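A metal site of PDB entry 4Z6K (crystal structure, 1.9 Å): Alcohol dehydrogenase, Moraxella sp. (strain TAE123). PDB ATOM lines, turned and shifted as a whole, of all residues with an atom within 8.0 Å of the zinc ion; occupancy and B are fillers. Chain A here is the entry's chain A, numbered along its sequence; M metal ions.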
ATOM      1  N   SER A  90       7.358 -19.865  25.682  1.00  0.00           N
ATOM      2  CA  SER A  90       6.251 -20.566  26.275  1.00  0.00           C
ATOM      3  C   SER A  90       5.241 -20.857  25.183  1.00  0.00           C
ATOM      4  O   SER A  90       5.239 -20.196  24.121  1.00  0.00           O
ATOM      5  CB  SER A  90       5.539 -19.756  27.389  1.00  0.00           C
ATOM      6  OG  SER A  90       4.917 -18.607  26.872  1.00  0.00           O
ATOM      7  N   ALA A  91       4.389 -21.796  25.486  1.00  0.00           N
ATOM      8  CA  ALA A  91       3.214 -22.157  24.622  1.00  0.00           C
ATOM      9  C   ALA A  91       2.106 -22.594  25.548  1.00  0.00           C
ATOM     10  O   ALA A  91       2.351 -22.731  26.729  1.00  0.00           O
ATOM     11  CB  ALA A  91       3.589 -23.275  23.706  1.00  0.00           C
ATOM     12  N   CYS A  92       0.910 -22.883  25.047  1.00  0.00           N
ATOM     13  CA  CYS A  92      -0.229 -22.801  25.976  1.00  0.00           C
ATOM     14  C   CYS A  92      -0.373 -24.142  26.682  1.00  0.00           C
ATOM     15  O   CYS A  92      -0.895 -24.254  27.770  1.00  0.00           O
ATOM     16  CB  CYS A  92      -1.510 -22.410  25.230  1.00  0.00           C
ATOM     17  SG  CYS A  92      -2.132 -23.661  24.041  1.00  0.00           S
ATOM     18  N   GLY A  93       0.066 -25.165  25.978  1.00  0.00           N
ATOM     19  CA  GLY A  93       0.045 -26.518  26.423  1.00  0.00           C
ATOM     20  C   GLY A  93      -1.275 -27.244  26.299  1.00  0.00           C
ATOM     21  O   GLY A  93      -1.368 -28.389  26.711  1.00  0.00           O
ATOM     22  N   HIS A  94      -2.297 -26.581  25.728  1.00  0.00           N
ATOM     23  CA  HIS A  94      -3.650 -27.112  25.711  1.00  0.00           C
ATOM     24  C   HIS A  94      -4.212 -27.267  24.301  1.00  0.00           C
ATOM     25  O   HIS A  94      -5.153 -27.969  24.130  1.00  0.00           O
ATOM     26  CB  HIS A  94      -4.653 -26.216  26.522  1.00  0.00           C
ATOM     27  CG  HIS A  94      -4.076 -25.587  27.733  1.00  0.00           C
ATOM     28  ND1 HIS A  94      -4.117 -24.221  27.944  1.00  0.00           N
ATOM     29  CD2 HIS A  94      -3.435 -26.117  28.822  1.00  0.00           C
ATOM     30  CE1 HIS A  94      -3.493 -23.940  29.082  1.00  0.00           C
ATOM     31  NE2 HIS A  94      -3.095 -25.069  29.645  1.00  0.00           N
ATOM     32  N   CYS A  95      -3.645 -26.601  23.306  1.00  0.00           N
ATOM     33  CA  CYS A  95      -4.238 -26.606  21.942  1.00  0.00           C
ATOM     34  C   CYS A  95      -3.823 -27.855  21.199  1.00  0.00           C
ATOM     35  O   CYS A  95      -2.911 -28.583  21.605  1.00  0.00           O
ATOM     36  CB  CYS A  95      -3.719 -25.278  21.285  1.00  0.00           C
ATOM     37  SG  CYS A  95      -2.129 -25.277  20.674  1.00  0.00           S
ATOM     38  N   THR A  96      -4.442 -28.121  20.079  1.00  0.00           N
ATOM     39  CA  THR A  96      -4.012 -29.213  19.224  1.00  0.00           C
ATOM     40  C   THR A  96      -2.545 -29.265  18.862  1.00  0.00           C
ATOM     41  O   THR A  96      -1.928 -30.328  18.911  1.00  0.00           O
ATOM     42  CB  THR A  96      -4.881 -29.239  17.979  1.00  0.00           C
ATOM     43  OG1 THR A  96      -6.240 -29.411  18.388  1.00  0.00           O
ATOM     44  CG2 THR A  96      -4.540 -30.386  17.064  1.00  0.00           C
ATOM     45  N   HIS A  97      -1.933 -28.118  18.534  1.00  0.00           N
ATOM     46  CA  HIS A  97      -0.602 -28.123  18.193  1.00  0.00           C
ATOM     47  C   HIS A  97       0.222 -28.529  19.422  1.00  0.00           C
ATOM     48  O   HIS A  97       1.158 -29.300  19.272  1.00  0.00           O
ATOM     49  CB  HIS A  97      -0.171 -26.685  17.794  1.00  0.00           C
ATOM     50  CG  HIS A  97      -0.844 -26.159  16.566  1.00  0.00           C
ATOM     51  ND1 HIS A  97      -0.886 -26.862  15.378  1.00  0.00           N
ATOM     52  CD2 HIS A  97      -1.399 -24.963  16.304  1.00  0.00           C
ATOM     53  CE1 HIS A  97      -1.448 -26.123  14.442  1.00  0.00           C
ATOM     54  NE2 HIS A  97      -1.787 -24.969  14.988  1.00  0.00           N
ATOM     55  N   CYS A  98      -0.003 -27.910  20.594  1.00  0.00           N
ATOM     56  CA  CYS A  98       0.753 -28.240  21.795  1.00  0.00           C
ATOM     57  C   CYS A  98       0.511 -29.712  22.193  1.00  0.00           C
ATOM     58  O   CYS A  98       1.484 -30.395  22.512  1.00  0.00           O
ATOM     59  CB  CYS A  98       0.346 -27.328  23.008  1.00  0.00           C
ATOM     60  SG  CYS A  98       0.919 -25.666  22.732  1.00  0.00           S
ATOM     61  N   LEU A  99      -0.672 -30.238  22.002  1.00  0.00           N
ATOM     62  CA  LEU A  99      -0.929 -31.621  22.503  1.00  0.00           C
ATOM     63  C   LEU A  99      -0.192 -32.664  21.627  1.00  0.00           C
ATOM     64  O   LEU A  99       0.025 -33.814  22.039  1.00  0.00           O
ATOM     65  CB  LEU A  99      -2.429 -31.906  22.583  1.00  0.00           C
ATOM     66  CG  LEU A  99      -3.246 -31.157  23.621  1.00  0.00           C
ATOM     67  CD1 LEU A  99      -4.719 -31.589  23.627  1.00  0.00           C
ATOM     68  CD2 LEU A  99      -2.606 -31.429  24.984  1.00  0.00           C
ATOM     69  N   TRP A 102       3.751 -30.286  18.509  1.00  0.00           N
ATOM     70  CA  TRP A 102       4.011 -29.239  17.543  1.00  0.00           C
ATOM     71  C   TRP A 102       3.773 -27.917  18.190  1.00  0.00           C
ATOM     72  O   TRP A 102       3.197 -26.988  17.624  1.00  0.00           O
ATOM     73  CB  TRP A 102       3.099 -29.416  16.344  1.00  0.00           C
ATOM     74  CG  TRP A 102       3.613 -30.422  15.352  1.00  0.00           C
ATOM     75  CD1 TRP A 102       3.155 -31.672  15.160  1.00  0.00           C
ATOM     76  CD2 TRP A 102       4.636 -30.215  14.346  1.00  0.00           C
ATOM     77  NE1 TRP A 102       3.819 -32.262  14.130  1.00  0.00           N
ATOM     78  CE2 TRP A 102       4.745 -31.394  13.628  1.00  0.00           C
ATOM     79  CE3 TRP A 102       5.441 -29.140  14.015  1.00  0.00           C
ATOM     80  CZ2 TRP A 102       5.639 -31.544  12.585  1.00  0.00           C
ATOM     81  CZ3 TRP A 102       6.356 -29.274  12.947  1.00  0.00           C
ATOM     82  CH2 TRP A 102       6.461 -30.454  12.290  1.00  0.00           C
ATOM     83  N   GLU A 103       4.425 -27.705  19.345  1.00  0.00           N
ATOM     84  CA  GLU A 103       4.190 -26.506  20.130  1.00  0.00           C
ATOM     85  C   GLU A 103       4.748 -25.276  19.424  1.00  0.00           C
ATOM     86  O   GLU A 103       4.390 -24.178  19.768  1.00  0.00           O
ATOM     87  CB  GLU A 103       4.722 -26.630  21.579  1.00  0.00           C
ATOM     88  CG  GLU A 103       6.206 -26.887  21.738  1.00  0.00           C
ATOM     89  CD  GLU A 103       6.580 -28.344  21.918  1.00  0.00           C
ATOM     90  OE1 GLU A 103       5.842 -29.257  21.378  1.00  0.00           O
ATOM     91  OE2 GLU A 103       7.630 -28.581  22.562  1.00  0.00           O
ATOM     92  N   THR A 104       5.686 -25.499  18.483  1.00  0.00           N
ATOM     93  CA  THR A 104       6.237 -24.431  17.707  1.00  0.00           C
ATOM     94  C   THR A 104       5.142 -23.710  16.903  1.00  0.00           C
ATOM     95  O   THR A 104       5.381 -22.582  16.433  1.00  0.00           O
ATOM     96  CB  THR A 104       7.333 -24.933  16.731  1.00  0.00           C
ATOM     97  OG1 THR A 104       6.860 -26.114  16.038  1.00  0.00           O
ATOM     98  CG2 THR A 104       8.565 -25.257  17.489  1.00  0.00           C
ATOM     99  N   LEU A 105       3.964 -24.328  16.770  1.00  0.00           N
ATOM    100  CA  LEU A 105       2.907 -23.773  15.958  1.00  0.00           C
ATOM    101  C   LEU A 105       1.877 -23.091  16.833  1.00  0.00           C
ATOM    102  O   LEU A 105       0.925 -22.485  16.317  1.00  0.00           O
ATOM    103  CB  LEU A 105       2.273 -24.815  15.092  1.00  0.00           C
ATOM    104  CG  LEU A 105       3.174 -25.526  14.059  1.00  0.00           C
ATOM    105  CD1 LEU A 105       2.338 -26.462  13.210  1.00  0.00           C
ATOM    106  CD2 LEU A 105       3.895 -24.509  13.194  1.00  0.00           C
ATOM    107  N   CYS A 106       2.111 -23.073  18.143  1.00  0.00           N
ATOM    108  CA  CYS A 106       1.054 -22.618  19.078  1.00  0.00           C
ATOM    109  C   CYS A 106       0.740 -21.123  18.828  1.00  0.00           C
ATOM    110  O   CYS A 106       1.649 -20.313  18.731  1.00  0.00           O
ATOM    111  CB  CYS A 106       1.434 -22.931  20.529  1.00  0.00           C
ATOM    112  SG  CYS A 106       0.310 -22.167  21.675  1.00  0.00           S
ATOM    113  N   GLU A 107      -0.541 -20.831  18.607  1.00  0.00           N
ATOM    114  CA  GLU A 107      -0.960 -19.505  18.245  1.00  0.00           C
ATOM    115  C   GLU A 107      -0.820 -18.505  19.415  1.00  0.00           C
ATOM    116  O   GLU A 107      -0.940 -17.345  19.195  1.00  0.00           O
ATOM    117  CB  GLU A 107      -2.393 -19.477  17.731  1.00  0.00           C
ATOM    118  CG  GLU A 107      -2.721 -20.304  16.480  1.00  0.00           C
ATOM    119  CD  GLU A 107      -2.335 -19.662  15.149  1.00  0.00           C
ATOM    120  OE1 GLU A 107      -1.707 -18.572  15.178  1.00  0.00           O
ATOM    121  OE2 GLU A 107      -2.658 -20.218  14.079  1.00  0.00           O
ATOM    122  N   SER A 108      -0.625 -18.955  20.646  1.00  0.00           N
ATOM    123  CA  SER A 108      -0.423 -18.074  21.741  1.00  0.00           C
ATOM    124  C   SER A 108       0.955 -18.182  22.352  1.00  0.00           C
ATOM    125  O   SER A 108       1.203 -17.824  23.492  1.00  0.00           O
ATOM    126  CB  SER A 108      -1.506 -18.187  22.788  1.00  0.00           C
ATOM    127  OG  SER A 108      -1.923 -19.482  22.995  1.00  0.00           O
ATOM    128  N   GLN A 109       1.894 -18.625  21.543  1.00  0.00           N
ATOM    129  CA  GLN A 109       3.220 -18.777  22.080  1.00  0.00           C
ATOM    130  C   GLN A 109       3.753 -17.434  22.391  1.00  0.00           C
ATOM    131  O   GLN A 109       3.336 -16.466  21.815  1.00  0.00           O
ATOM    132  CB  GLN A 109       4.196 -19.472  21.112  1.00  0.00           C
ATOM    133  CG  GLN A 109       4.539 -18.676  19.882  1.00  0.00           C
ATOM    134  CD  GLN A 109       5.264 -19.524  18.859  1.00  0.00           C
ATOM    135  OE1 GLN A 109       6.494 -19.425  18.735  1.00  0.00           O
ATOM    136  NE2 GLN A 109       4.542 -20.387  18.172  1.00  0.00           N
ATOM    137  N   TYR A 130       9.918 -24.620  29.367  1.00  0.00           N
ATOM    138  CA  TYR A 130      10.328 -24.423  28.023  1.00  0.00           C
ATOM    139  C   TYR A 130      11.859 -24.164  27.847  1.00  0.00           C
ATOM    140  O   TYR A 130      12.322 -24.022  26.750  1.00  0.00           O
ATOM    141  CB  TYR A 130       9.463 -23.303  27.407  1.00  0.00           C
ATOM    142  CG  TYR A 130       8.091 -23.769  27.191  1.00  0.00           C
ATOM    143  CD1 TYR A 130       7.157 -23.670  28.195  1.00  0.00           C
ATOM    144  CD2 TYR A 130       7.710 -24.454  26.032  1.00  0.00           C
ATOM    145  CE1 TYR A 130       5.932 -24.264  28.088  1.00  0.00           C
ATOM    146  CE2 TYR A 130       6.467 -25.013  25.895  1.00  0.00           C
ATOM    147  CZ  TYR A 130       5.541 -24.859  26.896  1.00  0.00           C
ATOM    148  OH  TYR A 130       4.261 -25.414  26.815  1.00  0.00           O
HETATM  149 ZN    ZN M   1      -0.798 -24.180  22.332  1.00  0.00          ZN
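Gly 93 touches the zinc ion (N to ZN, 3.9 Å).
Five residues have an atom within 4 Å of the zinc ion: Cys 92, Gly 93, Cys 95, Cys 98 and Cys 106.
O of Cys 92 lies close to NE2 of His 94, 3.0 Å away.
The side-chain sulfur of Cys 98 sits close to the backbone NH of Gly 93 (3.4 Å).
SG of Cys 106 lies close to N of Ser 108 (3.5 Å).
O of Cys 106 is in hydrogen-bond range of NE2 of Gln 109 (2.9 Å).
The side-chain sulfur (SG) of Cys 95 lies close to the backbone NH (N) of His 97 (3.6 Å).
The side-chain sulfur (SG) of Cys 92 is bound to the zinc ion.
The side-chain sulfur (SG) of Cys 98 binds the zinc ion.
The zinc ion is bound by SG of Cys 106, 2.4 Å away.
The side-chain sulfur (SG) of Cys 95 is bound to the zinc ion, 2.4 Å away.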
